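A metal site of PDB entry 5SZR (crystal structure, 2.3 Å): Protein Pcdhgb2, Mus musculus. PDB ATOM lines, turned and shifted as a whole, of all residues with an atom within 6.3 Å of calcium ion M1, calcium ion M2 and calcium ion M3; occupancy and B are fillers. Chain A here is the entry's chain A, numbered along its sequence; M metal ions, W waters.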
ATOM      1  N   GLU A 226     -21.549 -30.351   8.232  1.00  0.00           N
ATOM      2  CA  GLU A 226     -22.790 -30.547   7.513  1.00  0.00           C
ATOM      3  C   GLU A 226     -22.790 -29.819   6.178  1.00  0.00           C
ATOM      4  O   GLU A 226     -22.065 -28.845   5.985  1.00  0.00           O
ATOM      5  CB  GLU A 226     -23.938 -30.043   8.399  1.00  0.00           C
ATOM      6  CG  GLU A 226     -25.322 -30.120   7.876  1.00  0.00           C
ATOM      7  CD  GLU A 226     -26.316 -29.687   8.925  1.00  0.00           C
ATOM      8  OE1 GLU A 226     -26.066 -28.652   9.583  1.00  0.00           O
ATOM      9  OE2 GLU A 226     -27.316 -30.396   9.121  1.00  0.00           O
ATOM     10  N   ASN A 227     -23.610 -30.319   5.248  1.00  0.00           N
ATOM     11  CA  ASN A 227     -23.856 -29.709   3.947  1.00  0.00           C
ATOM     12  C   ASN A 227     -22.624 -29.712   3.056  1.00  0.00           C
ATOM     13  O   ASN A 227     -22.522 -28.936   2.105  1.00  0.00           O
ATOM     14  CB  ASN A 227     -24.405 -28.284   4.095  1.00  0.00           C
ATOM     15  CG  ASN A 227     -25.677 -28.240   4.918  1.00  0.00           C
ATOM     16  OD1 ASN A 227     -26.512 -29.142   4.831  1.00  0.00           O
ATOM     17  ND2 ASN A 227     -25.825 -27.207   5.735  1.00  0.00           N
ATOM     18  N   PHE A 283     -24.057 -34.472   4.132  1.00  0.00           N
ATOM     19  CA  PHE A 283     -24.556 -34.845   5.442  1.00  0.00           C
ATOM     20  C   PHE A 283     -25.487 -33.759   5.997  1.00  0.00           C
ATOM     21  O   PHE A 283     -25.305 -32.571   5.734  1.00  0.00           O
ATOM     22  CB  PHE A 283     -23.398 -35.093   6.411  1.00  0.00           C
ATOM     23  CG  PHE A 283     -22.514 -36.239   6.008  1.00  0.00           C
ATOM     24  CD1 PHE A 283     -21.154 -36.219   6.279  1.00  0.00           C
ATOM     25  CD2 PHE A 283     -23.035 -37.357   5.367  1.00  0.00           C
ATOM     26  CE1 PHE A 283     -20.324 -37.274   5.909  1.00  0.00           C
ATOM     27  CE2 PHE A 283     -22.211 -38.421   4.999  1.00  0.00           C
ATOM     28  CZ  PHE A 283     -20.862 -38.380   5.276  1.00  0.00           C
ATOM     29  N   ASP A 284     -26.476 -34.189   6.773  1.00  0.00           N
ATOM     30  CA  ASP A 284     -27.455 -33.295   7.399  1.00  0.00           C
ATOM     31  C   ASP A 284     -27.445 -33.586   8.894  1.00  0.00           C
ATOM     32  O   ASP A 284     -27.958 -34.619   9.335  1.00  0.00           O
ATOM     33  CB  ASP A 284     -28.841 -33.506   6.784  1.00  0.00           C
ATOM     34  CG  ASP A 284     -29.916 -32.651   7.446  1.00  0.00           C
ATOM     35  OD1 ASP A 284     -29.593 -31.682   8.157  1.00  0.00           O
ATOM     36  OD2 ASP A 284     -31.113 -32.942   7.211  1.00  0.00           O
ATOM     37  N   HIS A 285     -26.845 -32.672   9.663  1.00  0.00           N
ATOM     38  CA  HIS A 285     -26.701 -32.879  11.108  1.00  0.00           C
ATOM     39  C   HIS A 285     -28.045 -33.098  11.783  1.00  0.00           C
ATOM     40  O   HIS A 285     -28.128 -33.793  12.805  1.00  0.00           O
ATOM     41  CB  HIS A 285     -25.981 -31.683  11.728  1.00  0.00           C
ATOM     42  CG  HIS A 285     -25.949 -31.698  13.226  1.00  0.00           C
ATOM     43  ND1 HIS A 285     -24.958 -32.325  13.947  1.00  0.00           N
ATOM     44  CD2 HIS A 285     -26.796 -31.153  14.135  1.00  0.00           C
ATOM     45  CE1 HIS A 285     -25.195 -32.173  15.245  1.00  0.00           C
ATOM     46  NE2 HIS A 285     -26.300 -31.461  15.387  1.00  0.00           N
ATOM     47  N   GLU A 286     -29.119 -32.528  11.235  1.00  0.00           N
ATOM     48  CA  GLU A 286     -30.433 -32.664  11.846  1.00  0.00           C
ATOM     49  C   GLU A 286     -31.020 -34.072  11.652  1.00  0.00           C
ATOM     50  O   GLU A 286     -31.884 -34.466  12.443  1.00  0.00           O
ATOM     51  CB  GLU A 286     -31.374 -31.612  11.285  1.00  0.00           C
ATOM     52  CG  GLU A 286     -31.204 -30.218  11.932  1.00  0.00           C
ATOM     53  CD  GLU A 286     -29.876 -29.545  11.590  1.00  0.00           C
ATOM     54  OE1 GLU A 286     -29.514 -29.488  10.408  1.00  0.00           O
ATOM     55  OE2 GLU A 286     -29.196 -29.067  12.523  1.00  0.00           O
ATOM     56  N   GLN A 287     -30.562 -34.816  10.651  1.00  0.00           N
ATOM     57  CA  GLN A 287     -31.007 -36.198  10.472  1.00  0.00           C
ATOM     58  C   GLN A 287     -30.103 -37.190  11.207  1.00  0.00           C
ATOM     59  O   GLN A 287     -30.595 -38.095  11.884  1.00  0.00           O
ATOM     60  CB  GLN A 287     -31.082 -36.552   8.986  1.00  0.00           C
ATOM     61  CG  GLN A 287     -32.261 -35.908   8.261  1.00  0.00           C
ATOM     62  CD  GLN A 287     -33.599 -36.287   8.851  1.00  0.00           C
ATOM     63  OE1 GLN A 287     -33.855 -37.460   9.136  1.00  0.00           O
ATOM     64  NE2 GLN A 287     -34.454 -35.297   9.064  1.00  0.00           N
ATOM     65  N   GLY A 316     -20.907 -32.333  11.786  1.00  0.00           N
ATOM     66  CA  GLY A 316     -20.874 -31.067  12.494  1.00  0.00           C
ATOM     67  C   GLY A 316     -22.090 -30.211  12.184  1.00  0.00           C
ATOM     68  O   GLY A 316     -22.556 -30.152  11.053  1.00  0.00           O
ATOM     69  N   ASP A 317     -22.594 -29.538  13.216  1.00  0.00           N
ATOM     70  CA  ASP A 317     -23.758 -28.691  13.070  1.00  0.00           C
ATOM     71  C   ASP A 317     -23.376 -27.348  12.467  1.00  0.00           C
ATOM     72  O   ASP A 317     -22.429 -26.697  12.928  1.00  0.00           O
ATOM     73  CB  ASP A 317     -24.447 -28.488  14.425  1.00  0.00           C
ATOM     74  CG  ASP A 317     -25.706 -27.656  14.320  1.00  0.00           C
ATOM     75  OD1 ASP A 317     -26.411 -27.774  13.289  1.00  0.00           O
ATOM     76  OD2 ASP A 317     -26.004 -26.904  15.267  1.00  0.00           O
ATOM     77  N   ARG A 318     -24.084 -26.935  11.430  1.00  0.00           N
ATOM     78  CA  ARG A 318     -24.018 -25.585  10.897  1.00  0.00           C
ATOM     79  C   ARG A 318     -25.333 -24.863  11.132  1.00  0.00           C
ATOM     80  O   ARG A 318     -26.362 -25.486  11.443  1.00  0.00           O
ATOM     81  CB  ARG A 318     -23.688 -25.588   9.391  1.00  0.00           C
ATOM     82  CG  ARG A 318     -22.232 -25.847   9.054  1.00  0.00           C
ATOM     83  CD  ARG A 318     -21.972 -25.567   7.586  1.00  0.00           C
ATOM     84  NE  ARG A 318     -20.582 -25.785   7.212  1.00  0.00           N
ATOM     85  CZ  ARG A 318     -19.609 -24.888   7.405  1.00  0.00           C
ATOM     86  NH1 ARG A 318     -18.372 -25.168   7.035  1.00  0.00           N
ATOM     87  NH2 ARG A 318     -19.891 -23.724   7.972  1.00  0.00           N
ATOM     88  N   ASN A 319     -25.306 -23.548  10.982  1.00  0.00           N
ATOM     89  CA  ASN A 319     -26.503 -22.727  11.185  1.00  0.00           C
ATOM     90  C   ASN A 319     -27.254 -22.585   9.866  1.00  0.00           C
ATOM     91  O   ASN A 319     -27.326 -21.524   9.248  1.00  0.00           O
ATOM     92  CB  ASN A 319     -26.122 -21.360  11.764  1.00  0.00           C
ATOM     93  CG  ASN A 319     -27.338 -20.610  12.264  1.00  0.00           C
ATOM     94  OD1 ASN A 319     -28.256 -21.207  12.819  1.00  0.00           O
ATOM     95  ND2 ASN A 319     -27.372 -19.288  12.054  1.00  0.00           N
ATOM     96  N   ASP A 320     -27.851 -23.705   9.437  1.00  0.00           N
ATOM     97  CA  ASP A 320     -28.633 -23.723   8.211  1.00  0.00           C
ATOM     98  C   ASP A 320     -30.133 -23.690   8.462  1.00  0.00           C
ATOM     99  O   ASP A 320     -30.921 -23.954   7.544  1.00  0.00           O
ATOM    100  CB  ASP A 320     -28.250 -24.935   7.350  1.00  0.00           C
ATOM    101  CG  ASP A 320     -28.304 -26.249   8.121  1.00  0.00           C
ATOM    102  OD1 ASP A 320     -28.379 -26.225   9.358  1.00  0.00           O
ATOM    103  OD2 ASP A 320     -28.246 -27.315   7.461  1.00  0.00           O
ATOM    104  N   ASN A 321     -30.566 -23.369   9.679  1.00  0.00           N
ATOM    105  CA  ASN A 321     -31.977 -23.215   9.998  1.00  0.00           C
ATOM    106  C   ASN A 321     -32.168 -21.892  10.726  1.00  0.00           C
ATOM    107  O   ASN A 321     -31.520 -21.637  11.737  1.00  0.00           O
ATOM    108  CB  ASN A 321     -32.490 -24.368  10.861  1.00  0.00           C
ATOM    109  CG  ASN A 321     -32.541 -25.673  10.102  1.00  0.00           C
ATOM    110  OD1 ASN A 321     -33.541 -25.983   9.457  1.00  0.00           O
ATOM    111  ND2 ASN A 321     -31.468 -26.447  10.184  1.00  0.00           N
ATOM    112  N   ALA A 322     -33.049 -21.050  10.193  1.00  0.00           N
ATOM    113  CA  ALA A 322     -33.420 -19.823  10.873  1.00  0.00           C
ATOM    114  C   ALA A 322     -34.475 -20.110  11.928  1.00  0.00           C
ATOM    115  O   ALA A 322     -35.318 -21.001  11.736  1.00  0.00           O
ATOM    116  CB  ALA A 322     -33.941 -18.787   9.887  1.00  0.00           C
ATOM    117  N   PRO A 323     -34.459 -19.391  13.050  1.00  0.00           N
ATOM    118  CA  PRO A 323     -35.539 -19.553  14.025  1.00  0.00           C
ATOM    119  C   PRO A 323     -36.880 -19.189  13.411  1.00  0.00           C
ATOM    120  O   PRO A 323     -36.972 -18.384  12.486  1.00  0.00           O
ATOM    121  CB  PRO A 323     -35.149 -18.589  15.156  1.00  0.00           C
ATOM    122  CG  PRO A 323     -34.135 -17.672  14.577  1.00  0.00           C
ATOM    123  CD  PRO A 323     -33.438 -18.420  13.480  1.00  0.00           C
ATOM    124  N   ASP A 358     -35.844 -23.556  16.959  1.00  0.00           N
ATOM    125  CA  ASP A 358     -34.725 -23.538  16.028  1.00  0.00           C
ATOM    126  C   ASP A 358     -34.236 -24.972  15.845  1.00  0.00           C
ATOM    127  O   ASP A 358     -33.906 -25.641  16.825  1.00  0.00           O
ATOM    128  CB  ASP A 358     -33.593 -22.644  16.552  1.00  0.00           C
ATOM    129  CG  ASP A 358     -32.600 -22.268  15.468  1.00  0.00           C
ATOM    130  OD1 ASP A 358     -32.007 -23.169  14.838  1.00  0.00           O
ATOM    131  OD2 ASP A 358     -32.396 -21.057  15.250  1.00  0.00           O
ATOM    132  N   ALA A 359     -34.197 -25.436  14.595  1.00  0.00           N
ATOM    133  CA  ALA A 359     -33.885 -26.830  14.299  1.00  0.00           C
ATOM    134  C   ALA A 359     -32.435 -27.193  14.556  1.00  0.00           C
ATOM    135  O   ALA A 359     -32.098 -28.385  14.560  1.00  0.00           O
ATOM    136  CB  ALA A 359     -34.252 -27.161  12.856  1.00  0.00           C
ATOM    137  N   ASP A 360     -31.553 -26.215  14.755  1.00  0.00           N
ATOM    138  CA  ASP A 360     -30.129 -26.504  14.881  1.00  0.00           C
ATOM    139  C   ASP A 360     -29.774 -26.929  16.305  1.00  0.00           C
ATOM    140  O   ASP A 360     -30.671 -27.281  17.088  1.00  0.00           O
ATOM    141  CB  ASP A 360     -29.309 -25.281  14.456  1.00  0.00           C
ATOM    142  CG  ASP A 360     -29.528 -24.924  12.999  1.00  0.00           C
ATOM    143  OD1 ASP A 360     -29.664 -25.847  12.172  1.00  0.00           O
ATOM    144  OD2 ASP A 360     -29.554 -23.726  12.665  1.00  0.00           O
ATOM    145  N   SER A 361     -28.487 -26.906  16.641  1.00  0.00           N
ATOM    146  CA  SER A 361     -28.010 -27.318  17.951  1.00  0.00           C
ATOM    147  C   SER A 361     -27.024 -26.291  18.503  1.00  0.00           C
ATOM    148  O   SER A 361     -26.529 -25.429  17.764  1.00  0.00           O
ATOM    149  CB  SER A 361     -27.341 -28.703  17.899  1.00  0.00           C
ATOM    150  OG  SER A 361     -28.235 -29.668  17.378  1.00  0.00           O
ATOM    151  N   HIS A 363     -25.064 -23.247  20.014  1.00  0.00           N
ATOM    152  CA  HIS A 363     -25.268 -21.820  19.809  1.00  0.00           C
ATOM    153  C   HIS A 363     -26.081 -21.535  18.562  1.00  0.00           C
ATOM    154  O   HIS A 363     -26.761 -20.505  18.485  1.00  0.00           O
ATOM    155  CB  HIS A 363     -23.920 -21.093  19.742  1.00  0.00           C
ATOM    156  CG  HIS A 363     -23.261 -20.931  21.084  1.00  0.00           C
ATOM    157  ND1 HIS A 363     -22.515 -21.917  21.672  1.00  0.00           N
ATOM    158  CD2 HIS A 363     -23.248 -19.877  21.938  1.00  0.00           C
ATOM    159  CE1 HIS A 363     -22.058 -21.490  22.838  1.00  0.00           C
ATOM    160  NE2 HIS A 363     -22.490 -20.258  23.026  1.00  0.00           N
ATOM    161  N   ASN A 364     -26.033 -22.425  17.571  1.00  0.00           N
ATOM    162  CA  ASN A 364     -26.828 -22.224  16.364  1.00  0.00           C
ATOM    163  C   ASN A 364     -28.329 -22.228  16.656  1.00  0.00           C
ATOM    164  O   ASN A 364     -29.116 -21.742  15.832  1.00  0.00           O
ATOM    165  CB  ASN A 364     -26.501 -23.299  15.319  1.00  0.00           C
ATOM    166  CG  ASN A 364     -25.094 -23.156  14.762  1.00  0.00           C
ATOM    167  OD1 ASN A 364     -24.608 -22.060  14.534  1.00  0.00           O
ATOM    168  ND2 ASN A 364     -24.441 -24.298  14.517  1.00  0.00           N
ATOM    169  N   ALA A 365     -28.745 -22.737  17.829  1.00  0.00           N
ATOM    170  CA  ALA A 365     -30.158 -22.737  18.196  1.00  0.00           C
ATOM    171  C   ALA A 365     -30.406 -22.079  19.556  1.00  0.00           C
ATOM    172  O   ALA A 365     -31.473 -22.273  20.145  1.00  0.00           O
ATOM    173  CB  ALA A 365     -30.716 -24.167  18.201  1.00  0.00           C
ATOM    174  N   LEU A 367     -31.573 -19.119  21.366  1.00  0.00           N
ATOM    175  CA  LEU A 367     -32.360 -17.984  20.919  1.00  0.00           C
ATOM    176  C   LEU A 367     -32.288 -16.831  21.910  1.00  0.00           C
ATOM    177  O   LEU A 367     -32.225 -17.031  23.121  1.00  0.00           O
ATOM    178  CB  LEU A 367     -33.817 -18.401  20.701  1.00  0.00           C
ATOM    179  CG  LEU A 367     -33.920 -19.550  19.700  1.00  0.00           C
ATOM    180  CD1 LEU A 367     -35.361 -19.767  19.287  1.00  0.00           C
ATOM    181  CD2 LEU A 367     -33.014 -19.302  18.489  1.00  0.00           C
ATOM    182  N   ASP A 411     -30.728 -16.386  16.647  1.00  0.00           N
ATOM    183  CA  ASP A 411     -29.928 -17.464  17.192  1.00  0.00           C
ATOM    184  C   ASP A 411     -28.528 -16.954  17.495  1.00  0.00           C
ATOM    185  O   ASP A 411     -28.197 -15.785  17.269  1.00  0.00           O
ATOM    186  CB  ASP A 411     -29.931 -18.687  16.276  1.00  0.00           C
ATOM    187  CG  ASP A 411     -29.371 -18.401  14.881  1.00  0.00           C
ATOM    188  OD1 ASP A 411     -28.503 -17.516  14.722  1.00  0.00           O
ATOM    189  OD2 ASP A 411     -29.799 -19.085  13.931  1.00  0.00           O
ATOM    190  N   GLY A 412     -27.677 -17.828  18.018  1.00  0.00           N
ATOM    191  CA  GLY A 412     -26.335 -17.427  18.402  1.00  0.00           C
ATOM    192  C   GLY A 412     -25.291 -17.811  17.379  1.00  0.00           C
ATOM    193  O   GLY A 412     -24.094 -17.825  17.689  1.00  0.00           O
ATOM    194  N   GLY A 413     -25.724 -18.123  16.162  1.00  0.00           N
ATOM    195  CA  GLY A 413     -24.820 -18.492  15.103  1.00  0.00           C
ATOM    196  C   GLY A 413     -24.068 -17.307  14.526  1.00  0.00           C
ATOM    197  O   GLY A 413     -24.278 -16.147  14.893  1.00  0.00           O
ATOM    198  N   LEU A 417     -28.980 -15.910  12.148  1.00  0.00           N
ATOM    199  CA  LEU A 417     -30.287 -15.892  11.493  1.00  0.00           C
ATOM    200  C   LEU A 417     -31.359 -15.463  12.487  1.00  0.00           C
ATOM    201  O   LEU A 417     -31.208 -15.630  13.705  1.00  0.00           O
ATOM    202  CB  LEU A 417     -30.620 -17.275  10.916  1.00  0.00           C
ATOM    203  CG  LEU A 417     -29.601 -17.889   9.961  1.00  0.00           C
ATOM    204  CD1 LEU A 417     -30.017 -19.292   9.559  1.00  0.00           C
ATOM    205  CD2 LEU A 417     -29.418 -17.015   8.723  1.00  0.00           C
HETATM  206 CA    CA M   1     -29.117 -29.364   8.134  1.00  0.00          CA
HETATM  207 CA    CA M   2     -27.914 -27.455  11.365  1.00  0.00          CA
HETATM  208 CA    CA M   3     -30.267 -21.671  13.792  1.00  0.00          CA
HETATM  209  O   HOH W   1     -28.849 -30.056   5.853  1.00  0.00           O
HETATM  210  O   HOH W   2     -31.574 -28.600   7.853  1.00  0.00           O
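The side-chain carboxylate (OD2) of Asp 317 is in hydrogen-bond range of the backbone NH (N) of Ser 361.
The side-chain carboxylate (OD1) of Asp 411 is in hydrogen-bond range of the backbone NH (N) of Gly 413 (3.2 Å).
The side-chain carboxylate of Asp 320 sits close to the side-chain amide nitrogen of Asn 321.
The side-chain carboxylate of Asp 320 lies close to the side-chain amide nitrogen of Asn 227, 3.0 Å away.
The side-chain carboxylate (OD2) of Asp 317 sits at hydrogen-bond distance from the side-chain amide nitrogen (ND2) of Asn 364 (3.1 Å).
The backbone NH (N) of Leu 417 lies within hydrogen-bond range of the side-chain carboxylate (OD1) of Asp 411 (3.1 Å).
The backbone NH of Glu 226 sits close to the backbone carbonyl oxygen of Gly 316, at 3.0 Å.
Four residues have an atom within 4 Å of calcium ion M1: Glu 226, Asp 284, Glu 286 and Asp 320.
Along chain A the residues within 4 Å of calcium ion M1 span positions 226 to 320.
Within 4 Å of calcium ion M2: Glu 226, Glu 286, Asp 317, Arg 318, Asp 320, Asn 321 and Asp 360.
Along chain A the residues within 4 Å of calcium ion M2 span positions 226 to 360.
Within 4 Å of calcium ion M3: Asn 319, Asn 321, Asp 358, Asp 360, Asn 364 and Asp 411.
OE2 of Glu 226 binds calcium ion M1 (2.3 Å).
OE1 of Glu 286 binds calcium ion M1 (2.3 Å).
OD2 of Asp 320 is bound to calcium ion M1 (2.3 Å).
Calcium ion M1 is bound by OD1 of Asp 284 (2.4 Å).
Water W1 is bound to calcium ion M1 (2.4 Å).
Water W2 is bound to calcium ion M1 (2.6 Å).
Calcium ion M1 has six donor atoms within binding distance.
Calcium ion M2 is bound by OE2 of Glu 286 (2.4 Å), OD1 of Asp 320 (2.4 Å), OD1 of Asp 317 (2.5 Å), O of Arg 318 (2.5 Å), OD1 of Asp 360 (2.5 Å), OE1 of Glu 286 (2.8 Å) and OE1 of Glu 226 (2.8 Å).
Calcium ion M2 has seven donor atoms within binding distance.
Calcium ion M3 is bound by OD1 of Asn 319, O of Asn 364, O of Asn 321, OD2 of Asp 360, OD1 of Asp 358, OD2 of Asp 411 and OD2 of Asp 358.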
